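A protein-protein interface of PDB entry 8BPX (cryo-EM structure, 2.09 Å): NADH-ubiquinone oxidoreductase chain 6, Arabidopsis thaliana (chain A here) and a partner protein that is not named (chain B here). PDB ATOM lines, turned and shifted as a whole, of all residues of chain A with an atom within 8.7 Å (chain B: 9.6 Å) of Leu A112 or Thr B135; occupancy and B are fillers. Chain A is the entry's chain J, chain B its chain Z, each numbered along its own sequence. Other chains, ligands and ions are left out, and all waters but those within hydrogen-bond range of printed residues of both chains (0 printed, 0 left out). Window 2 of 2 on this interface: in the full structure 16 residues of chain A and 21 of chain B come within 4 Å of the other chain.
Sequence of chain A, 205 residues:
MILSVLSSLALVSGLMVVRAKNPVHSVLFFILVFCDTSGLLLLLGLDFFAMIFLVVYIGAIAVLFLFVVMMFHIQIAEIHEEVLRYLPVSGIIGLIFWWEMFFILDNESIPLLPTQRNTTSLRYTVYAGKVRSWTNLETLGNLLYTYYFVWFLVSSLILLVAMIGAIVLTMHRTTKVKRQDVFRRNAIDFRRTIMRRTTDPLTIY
Leu A112 touches just one residue of chain B: Thr B135 (3.7 Å).
Thr B135 touches just one residue of chain A: Leu A112.
No residue of chain B comes within 4 Å of Pro A111.
No residue of chain A comes within 4 Å of Ala B134.
No residue of chain A comes within 4 Å of Gly B136.
Glu B137 touches one residue of chain A.
Printed residues of chain A within 4 Å of Tyr B104: Leu A122 (3.8 Å).
Of the printed residues of chain B, Leu A122 touches Phe B97, Tyr B104 and Pro B133.
Of the printed residues of chain B, Tyr A124 touches Phe B97 (3.98 Å).
Printed residues of chain A within 4 Å of Pro B133: Leu A122 (3.7 Å).
Of the printed residues of chain A, Phe B97 touches Leu A122 and Tyr A124.
Arg B139 touches none of the printed residues of chain A.
The nearest residue of chain B that does not touch Leu A112 is Ala B134 (4.4 Å).
The nearest printed residue of chain B that does not touch Tyr A124 is Pro B132 (4.003 Å).
NH2 of Arg A123 lies within salt-bridge range of OE1 of Glu B137.
Of the 12 printed residues of chain A, 4 touch a printed residue of chain B.
Printed residues of chain A that touch a printed residue of chain B: Leu A112, Leu A122, Arg A123 and Tyr A124.
Of the 13 printed residues of chain B, 5 touch a printed residue of chain A.
Printed residues of chain B that touch a printed residue of chain A: Phe B97, Tyr B104, Pro B133, Thr B135 and Glu B137.
Among the printed residues, 6 pairs touch across the chains.
Among the printed residues, Asp or Glu carboxylates within 4 Å of a Lys or Arg side-chain nitrogen of the other chain: Arg A123 with Glu B137 (3.2 Å).
The side-chain carboxylate (OE1) of Glu B137 sits at hydrogen-bond distance from the side-chain hydroxyl (OG1) of Thr B135 (3.2 Å).
Leu A112 touches Thr B135.
Phe B97 touches Leu A122.
Leu A122 touches Tyr B104.
CG of Pro B133 touches O of Leu A122, at 3.7 Å.
Tyr A124 touches Phe B97.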
ATOM      1  N   SER A 109      30.127   1.251  27.937  1.00  0.00           N
ATOM      2  CA  SER A 109      28.743   0.848  27.706  1.00  0.00           C
ATOM      3  C   SER A 109      28.607  -0.608  28.139  1.00  0.00           C
ATOM      4  O   SER A 109      28.741  -1.529  27.330  1.00  0.00           O
ATOM      5  CB  SER A 109      28.363   1.047  26.251  1.00  0.00           C
ATOM      6  OG  SER A 109      28.315   2.427  25.933  1.00  0.00           O
ATOM      7  N   ILE A 110      28.342  -0.806  29.421  1.00  0.00           N
ATOM      8  CA  ILE A 110      28.207  -2.154  29.977  1.00  0.00           C
ATOM      9  C   ILE A 110      26.841  -2.710  29.588  1.00  0.00           C
ATOM     10  O   ILE A 110      25.822  -2.049  29.829  1.00  0.00           O
ATOM     11  CB  ILE A 110      28.381  -2.125  31.491  1.00  0.00           C
ATOM     12  CG1 ILE A 110      29.842  -1.848  31.846  1.00  0.00           C
ATOM     13  CG2 ILE A 110      27.925  -3.438  32.108  1.00  0.00           C
ATOM     14  CD1 ILE A 110      30.030  -1.233  33.190  1.00  0.00           C
ATOM     15  N   PRO A 111      26.776  -3.895  28.994  1.00  0.00           N
ATOM     16  CA  PRO A 111      25.482  -4.437  28.571  1.00  0.00           C
ATOM     17  C   PRO A 111      24.590  -4.786  29.751  1.00  0.00           C
ATOM     18  O   PRO A 111      25.052  -5.146  30.835  1.00  0.00           O
ATOM     19  CB  PRO A 111      25.863  -5.689  27.777  1.00  0.00           C
ATOM     20  CG  PRO A 111      27.187  -6.080  28.304  1.00  0.00           C
ATOM     21  CD  PRO A 111      27.888  -4.804  28.678  1.00  0.00           C
ATOM     22  N   LEU A 112      23.287  -4.670  29.519  1.00  0.00           N
ATOM     23  CA  LEU A 112      22.292  -5.125  30.478  1.00  0.00           C
ATOM     24  C   LEU A 112      22.035  -6.611  30.256  1.00  0.00           C
ATOM     25  O   LEU A 112      21.529  -7.005  29.201  1.00  0.00           O
ATOM     26  CB  LEU A 112      21.005  -4.320  30.324  1.00  0.00           C
ATOM     27  CG  LEU A 112      19.899  -4.543  31.353  1.00  0.00           C
ATOM     28  CD1 LEU A 112      20.312  -4.019  32.723  1.00  0.00           C
ATOM     29  CD2 LEU A 112      18.608  -3.896  30.887  1.00  0.00           C
ATOM     30  N   LEU A 113      22.389  -7.432  31.238  1.00  0.00           N
ATOM     31  CA  LEU A 113      22.160  -8.866  31.117  1.00  0.00           C
ATOM     32  C   LEU A 113      20.663  -9.156  31.160  1.00  0.00           C
ATOM     33  O   LEU A 113      19.977  -8.709  32.085  1.00  0.00           O
ATOM     34  CB  LEU A 113      22.887  -9.626  32.224  1.00  0.00           C
ATOM     35  CG  LEU A 113      24.377  -9.306  32.349  1.00  0.00           C
ATOM     36  CD1 LEU A 113      25.019 -10.080  33.482  1.00  0.00           C
ATOM     37  CD2 LEU A 113      25.086  -9.592  31.033  1.00  0.00           C
ATOM     38  N   PRO A 114      20.123  -9.889  30.189  1.00  0.00           N
ATOM     39  CA  PRO A 114      18.676 -10.158  30.173  1.00  0.00           C
ATOM     40  C   PRO A 114      18.315 -11.186  31.235  1.00  0.00           C
ATOM     41  O   PRO A 114      18.846 -12.299  31.247  1.00  0.00           O
ATOM     42  CB  PRO A 114      18.431 -10.690  28.757  1.00  0.00           C
ATOM     43  CG  PRO A 114      19.732 -11.301  28.359  1.00  0.00           C
ATOM     44  CD  PRO A 114      20.831 -10.581  29.098  1.00  0.00           C
ATOM     45  N   THR A 115      17.411 -10.806  32.128  1.00  0.00           N
ATOM     46  CA  THR A 115      17.068 -11.609  33.291  1.00  0.00           C
ATOM     47  C   THR A 115      15.796 -12.413  33.044  1.00  0.00           C
ATOM     48  O   THR A 115      15.077 -12.211  32.063  1.00  0.00           O
ATOM     49  CB  THR A 115      16.898 -10.717  34.525  1.00  0.00           C
ATOM     50  OG1 THR A 115      15.789  -9.830  34.328  1.00  0.00           O
ATOM     51  CG2 THR A 115      18.152  -9.900  34.760  1.00  0.00           C
ATOM     52  N   THR A 119      11.023  -7.217  32.234  1.00  0.00           N
ATOM     53  CA  THR A 119      11.342  -5.805  32.378  1.00  0.00           C
ATOM     54  C   THR A 119      10.519  -4.925  31.445  1.00  0.00           C
ATOM     55  O   THR A 119      10.534  -3.699  31.598  1.00  0.00           O
ATOM     56  CB  THR A 119      12.836  -5.576  32.126  1.00  0.00           C
ATOM     57  OG1 THR A 119      13.581  -6.687  32.637  1.00  0.00           O
ATOM     58  CG2 THR A 119      13.315  -4.309  32.824  1.00  0.00           C
ATOM     59  N   THR A 120       9.789  -5.523  30.497  1.00  0.00           N
ATOM     60  CA  THR A 120       9.017  -4.736  29.540  1.00  0.00           C
ATOM     61  C   THR A 120       7.976  -3.862  30.229  1.00  0.00           C
ATOM     62  O   THR A 120       7.616  -2.801  29.708  1.00  0.00           O
ATOM     63  CB  THR A 120       8.339  -5.655  28.524  1.00  0.00           C
ATOM     64  OG1 THR A 120       7.368  -6.473  29.189  1.00  0.00           O
ATOM     65  CG2 THR A 120       9.366  -6.546  27.842  1.00  0.00           C
ATOM     66  N   LEU A 122       8.414  -2.112  32.810  1.00  0.00           N
ATOM     67  CA  LEU A 122       9.066  -0.913  33.313  1.00  0.00           C
ATOM     68  C   LEU A 122       9.363   0.105  32.223  1.00  0.00           C
ATOM     69  O   LEU A 122       9.949   1.151  32.515  1.00  0.00           O
ATOM     70  CB  LEU A 122      10.355  -1.281  34.054  1.00  0.00           C
ATOM     71  CG  LEU A 122      10.134  -1.983  35.397  1.00  0.00           C
ATOM     72  CD1 LEU A 122      11.373  -1.899  36.265  1.00  0.00           C
ATOM     73  CD2 LEU A 122       8.944  -1.375  36.119  1.00  0.00           C
ATOM     74  N   ARG A 123       8.982  -0.177  30.980  1.00  0.00           N
ATOM     75  CA  ARG A 123       9.084   0.816  29.921  1.00  0.00           C
ATOM     76  C   ARG A 123       8.065   1.923  30.167  1.00  0.00           C
ATOM     77  O   ARG A 123       6.858   1.666  30.213  1.00  0.00           O
ATOM     78  CB  ARG A 123       8.858   0.164  28.558  1.00  0.00           C
ATOM     79  CG  ARG A 123       9.851   0.594  27.489  1.00  0.00           C
ATOM     80  CD  ARG A 123      10.115  -0.516  26.481  1.00  0.00           C
ATOM     81  NE  ARG A 123      10.982  -1.557  27.019  1.00  0.00           N
ATOM     82  CZ  ARG A 123      11.284  -2.683  26.386  1.00  0.00           C
ATOM     83  NH1 ARG A 123      10.807  -2.947  25.180  1.00  0.00           N
ATOM     84  NH2 ARG A 123      12.087  -3.564  26.975  1.00  0.00           N
ATOM     85  N   TYR A 124       8.548   3.149  30.337  1.00  0.00           N
ATOM     86  CA  TYR A 124       7.686   4.298  30.580  1.00  0.00           C
ATOM     87  C   TYR A 124       7.368   4.986  29.258  1.00  0.00           C
ATOM     88  O   TYR A 124       8.275   5.289  28.478  1.00  0.00           O
ATOM     89  CB  TYR A 124       8.359   5.277  31.544  1.00  0.00           C
ATOM     90  CG  TYR A 124       7.510   6.474  31.909  1.00  0.00           C
ATOM     91  CD1 TYR A 124       6.209   6.313  32.372  1.00  0.00           C
ATOM     92  CD2 TYR A 124       8.008   7.764  31.790  1.00  0.00           C
ATOM     93  CE1 TYR A 124       5.433   7.399  32.705  1.00  0.00           C
ATOM     94  CE2 TYR A 124       7.236   8.858  32.119  1.00  0.00           C
ATOM     95  CZ  TYR A 124       5.949   8.669  32.575  1.00  0.00           C
ATOM     96  OH  TYR A 124       5.181   9.756  32.902  1.00  0.00           O
ATOM     97  N   PHE B  97       2.818   2.715  35.649  1.00  0.00           N
ATOM     98  CA  PHE B  97       4.251   2.650  35.895  1.00  0.00           C
ATOM     99  C   PHE B  97       4.564   2.689  37.383  1.00  0.00           C
ATOM    100  O   PHE B  97       5.495   2.022  37.836  1.00  0.00           O
ATOM    101  CB  PHE B  97       4.984   3.784  35.184  1.00  0.00           C
ATOM    102  CG  PHE B  97       6.461   3.782  35.438  1.00  0.00           C
ATOM    103  CD1 PHE B  97       7.303   2.980  34.687  1.00  0.00           C
ATOM    104  CD2 PHE B  97       7.007   4.547  36.454  1.00  0.00           C
ATOM    105  CE1 PHE B  97       8.661   2.961  34.927  1.00  0.00           C
ATOM    106  CE2 PHE B  97       8.362   4.527  36.702  1.00  0.00           C
ATOM    107  CZ  PHE B  97       9.190   3.737  35.934  1.00  0.00           C
ATOM    108  N   TYR B 104       8.460  -3.917  41.419  1.00  0.00           N
ATOM    109  CA  TYR B 104       9.867  -4.197  41.155  1.00  0.00           C
ATOM    110  C   TYR B 104      10.738  -3.846  42.356  1.00  0.00           C
ATOM    111  O   TYR B 104      11.738  -4.518  42.623  1.00  0.00           O
ATOM    112  CB  TYR B 104      10.339  -3.440  39.912  1.00  0.00           C
ATOM    113  CG  TYR B 104      11.837  -3.491  39.723  1.00  0.00           C
ATOM    114  CD1 TYR B 104      12.448  -4.608  39.172  1.00  0.00           C
ATOM    115  CD2 TYR B 104      12.641  -2.428  40.109  1.00  0.00           C
ATOM    116  CE1 TYR B 104      13.814  -4.661  39.006  1.00  0.00           C
ATOM    117  CE2 TYR B 104      14.006  -2.473  39.947  1.00  0.00           C
ATOM    118  CZ  TYR B 104      14.588  -3.591  39.396  1.00  0.00           C
ATOM    119  OH  TYR B 104      15.951  -3.636  39.233  1.00  0.00           O
ATOM    120  N   MET B 131      14.631   9.893  35.967  1.00  0.00           N
ATOM    121  CA  MET B 131      14.744   9.410  34.603  1.00  0.00           C
ATOM    122  C   MET B 131      14.057   8.058  34.497  1.00  0.00           C
ATOM    123  O   MET B 131      14.083   7.271  35.448  1.00  0.00           O
ATOM    124  CB  MET B 131      16.213   9.276  34.170  1.00  0.00           C
ATOM    125  CG  MET B 131      17.001  10.582  34.200  1.00  0.00           C
ATOM    126  SD  MET B 131      16.615  11.709  32.847  1.00  0.00           S
ATOM    127  CE  MET B 131      16.976  10.687  31.423  1.00  0.00           C
ATOM    128  N   PRO B 132      13.427   7.765  33.361  1.00  0.00           N
ATOM    129  CA  PRO B 132      12.840   6.442  33.180  1.00  0.00           C
ATOM    130  C   PRO B 132      13.919   5.382  33.183  1.00  0.00           C
ATOM    131  O   PRO B 132      15.084   5.652  32.833  1.00  0.00           O
ATOM    132  CB  PRO B 132      12.148   6.541  31.810  1.00  0.00           C
ATOM    133  CG  PRO B 132      12.185   7.965  31.409  1.00  0.00           C
ATOM    134  CD  PRO B 132      13.241   8.648  32.198  1.00  0.00           C
ATOM    135  N   PRO B 133      13.588   4.157  33.587  1.00  0.00           N
ATOM    136  CA  PRO B 133      14.600   3.092  33.590  1.00  0.00           C
ATOM    137  C   PRO B 133      15.102   2.811  32.179  1.00  0.00           C
ATOM    138  O   PRO B 133      14.320   2.688  31.233  1.00  0.00           O
ATOM    139  CB  PRO B 133      13.857   1.887  34.180  1.00  0.00           C
ATOM    140  CG  PRO B 133      12.569   2.421  34.729  1.00  0.00           C
ATOM    141  CD  PRO B 133      12.255   3.657  33.957  1.00  0.00           C
ATOM    142  N   ALA B 134      16.420   2.724  32.045  1.00  0.00           N
ATOM    143  CA  ALA B 134      17.021   2.412  30.758  1.00  0.00           C
ATOM    144  C   ALA B 134      16.733   0.961  30.388  1.00  0.00           C
ATOM    145  O   ALA B 134      16.650   0.081  31.248  1.00  0.00           O
ATOM    146  CB  ALA B 134      18.526   2.672  30.795  1.00  0.00           C
ATOM    147  N   THR B 135      16.579   0.713  29.089  1.00  0.00           N
ATOM    148  CA  THR B 135      16.074  -0.568  28.620  1.00  0.00           C
ATOM    149  C   THR B 135      17.115  -1.456  27.956  1.00  0.00           C
ATOM    150  O   THR B 135      16.908  -2.670  27.891  1.00  0.00           O
ATOM    151  CB  THR B 135      14.915  -0.351  27.639  1.00  0.00           C
ATOM    152  OG1 THR B 135      15.435  -0.094  26.330  1.00  0.00           O
ATOM    153  CG2 THR B 135      14.071   0.828  28.082  1.00  0.00           C
ATOM    154  N   GLY B 136      18.193  -0.887  27.474  1.00  0.00           N
ATOM    155  CA  GLY B 136      19.245  -1.703  26.827  1.00  0.00           C
ATOM    156  C   GLY B 136      18.870  -2.175  25.427  1.00  0.00           C
ATOM    157  O   GLY B 136      19.468  -3.120  24.949  1.00  0.00           O
ATOM    158  N   GLU B 137      17.924  -1.499  24.782  1.00  0.00           N
ATOM    159  CA  GLU B 137      17.539  -1.805  23.382  1.00  0.00           C
ATOM    160  C   GLU B 137      17.734  -0.455  22.684  1.00  0.00           C
ATOM    161  O   GLU B 137      17.322   0.530  23.235  1.00  0.00           O
ATOM    162  CB  GLU B 137      16.133  -2.379  23.223  1.00  0.00           C
ATOM    163  CG  GLU B 137      15.974  -3.786  23.734  1.00  0.00           C
ATOM    164  CD  GLU B 137      15.906  -3.843  25.247  1.00  0.00           C
ATOM    165  OE1 GLU B 137      14.998  -3.204  25.814  1.00  0.00           O
ATOM    166  OE2 GLU B 137      16.787  -4.485  25.850  1.00  0.00           O
ATOM    167  N   LEU B 138      18.446  -0.465  21.570  1.00  0.00           N
ATOM    168  CA  LEU B 138      18.817   0.824  20.949  1.00  0.00           C
ATOM    169  C   LEU B 138      17.587   1.611  20.503  1.00  0.00           C
ATOM    170  O   LEU B 138      17.503   2.766  20.881  1.00  0.00           O
ATOM    171  CB  LEU B 138      19.803   0.526  19.836  1.00  0.00           C
ATOM    172  CG  LEU B 138      21.004   1.460  19.785  1.00  0.00           C
ATOM    173  CD1 LEU B 138      21.679   1.560  21.138  1.00  0.00           C
ATOM    174  CD2 LEU B 138      21.978   1.000  18.730  1.00  0.00           C
ATOM    175  N   ARG B 139      16.686   1.027  19.730  1.00  0.00           N
ATOM    176  CA  ARG B 139      15.534   1.731  19.161  1.00  0.00           C
ATOM    177  C   ARG B 139      14.267   0.904  19.350  1.00  0.00           C
ATOM    178  O   ARG B 139      13.696   0.377  18.390  1.00  0.00           O
ATOM    179  CB  ARG B 139      15.771   2.047  17.682  1.00  0.00           C
ATOM    180  CG  ARG B 139      14.871   3.135  17.137  1.00  0.00           C
ATOM    181  CD  ARG B 139      15.564   4.479  17.155  1.00  0.00           C
ATOM    182  NE  ARG B 139      14.625   5.581  17.003  1.00  0.00           N
ATOM    183  CZ  ARG B 139      14.353   6.182  15.854  1.00  0.00           C
ATOM    184  NH1 ARG B 139      14.926   5.803  14.722  1.00  0.00           N
ATOM    185  NH2 ARG B 139      13.483   7.187  15.837  1.00  0.00           N
ATOM    186  N   PRO B 140      13.785   0.785  20.591  1.00  0.00           N
ATOM    187  CA  PRO B 140      12.578  -0.024  20.822  1.00  0.00           C
ATOM    188  C   PRO B 140      11.295   0.626  20.328  1.00  0.00           C
ATOM    189  O   PRO B 140      10.332  -0.089  20.033  1.00  0.00           O
ATOM    190  CB  PRO B 140      12.565  -0.201  22.345  1.00  0.00           C
ATOM    191  CG  PRO B 140      13.287   0.981  22.871  1.00  0.00           C
ATOM    192  CD  PRO B 140      14.268   1.437  21.822  1.00  0.00           C
ATOM    193  N   ASP B 141      11.253   1.956  20.215  1.00  0.00           N
ATOM    194  CA  ASP B 141       9.991   2.644  19.954  1.00  0.00           C
ATOM    195  C   ASP B 141       9.498   2.495  18.518  1.00  0.00           C
ATOM    196  O   ASP B 141       8.319   2.754  18.261  1.00  0.00           O
ATOM    197  CB  ASP B 141      10.127   4.130  20.288  1.00  0.00           C
ATOM    198  CG  ASP B 141       8.798   4.772  20.634  1.00  0.00           C
ATOM    199  OD1 ASP B 141       8.097   5.230  19.706  1.00  0.00           O
ATOM    200  OD2 ASP B 141       8.457   4.822  21.834  1.00  0.00           O
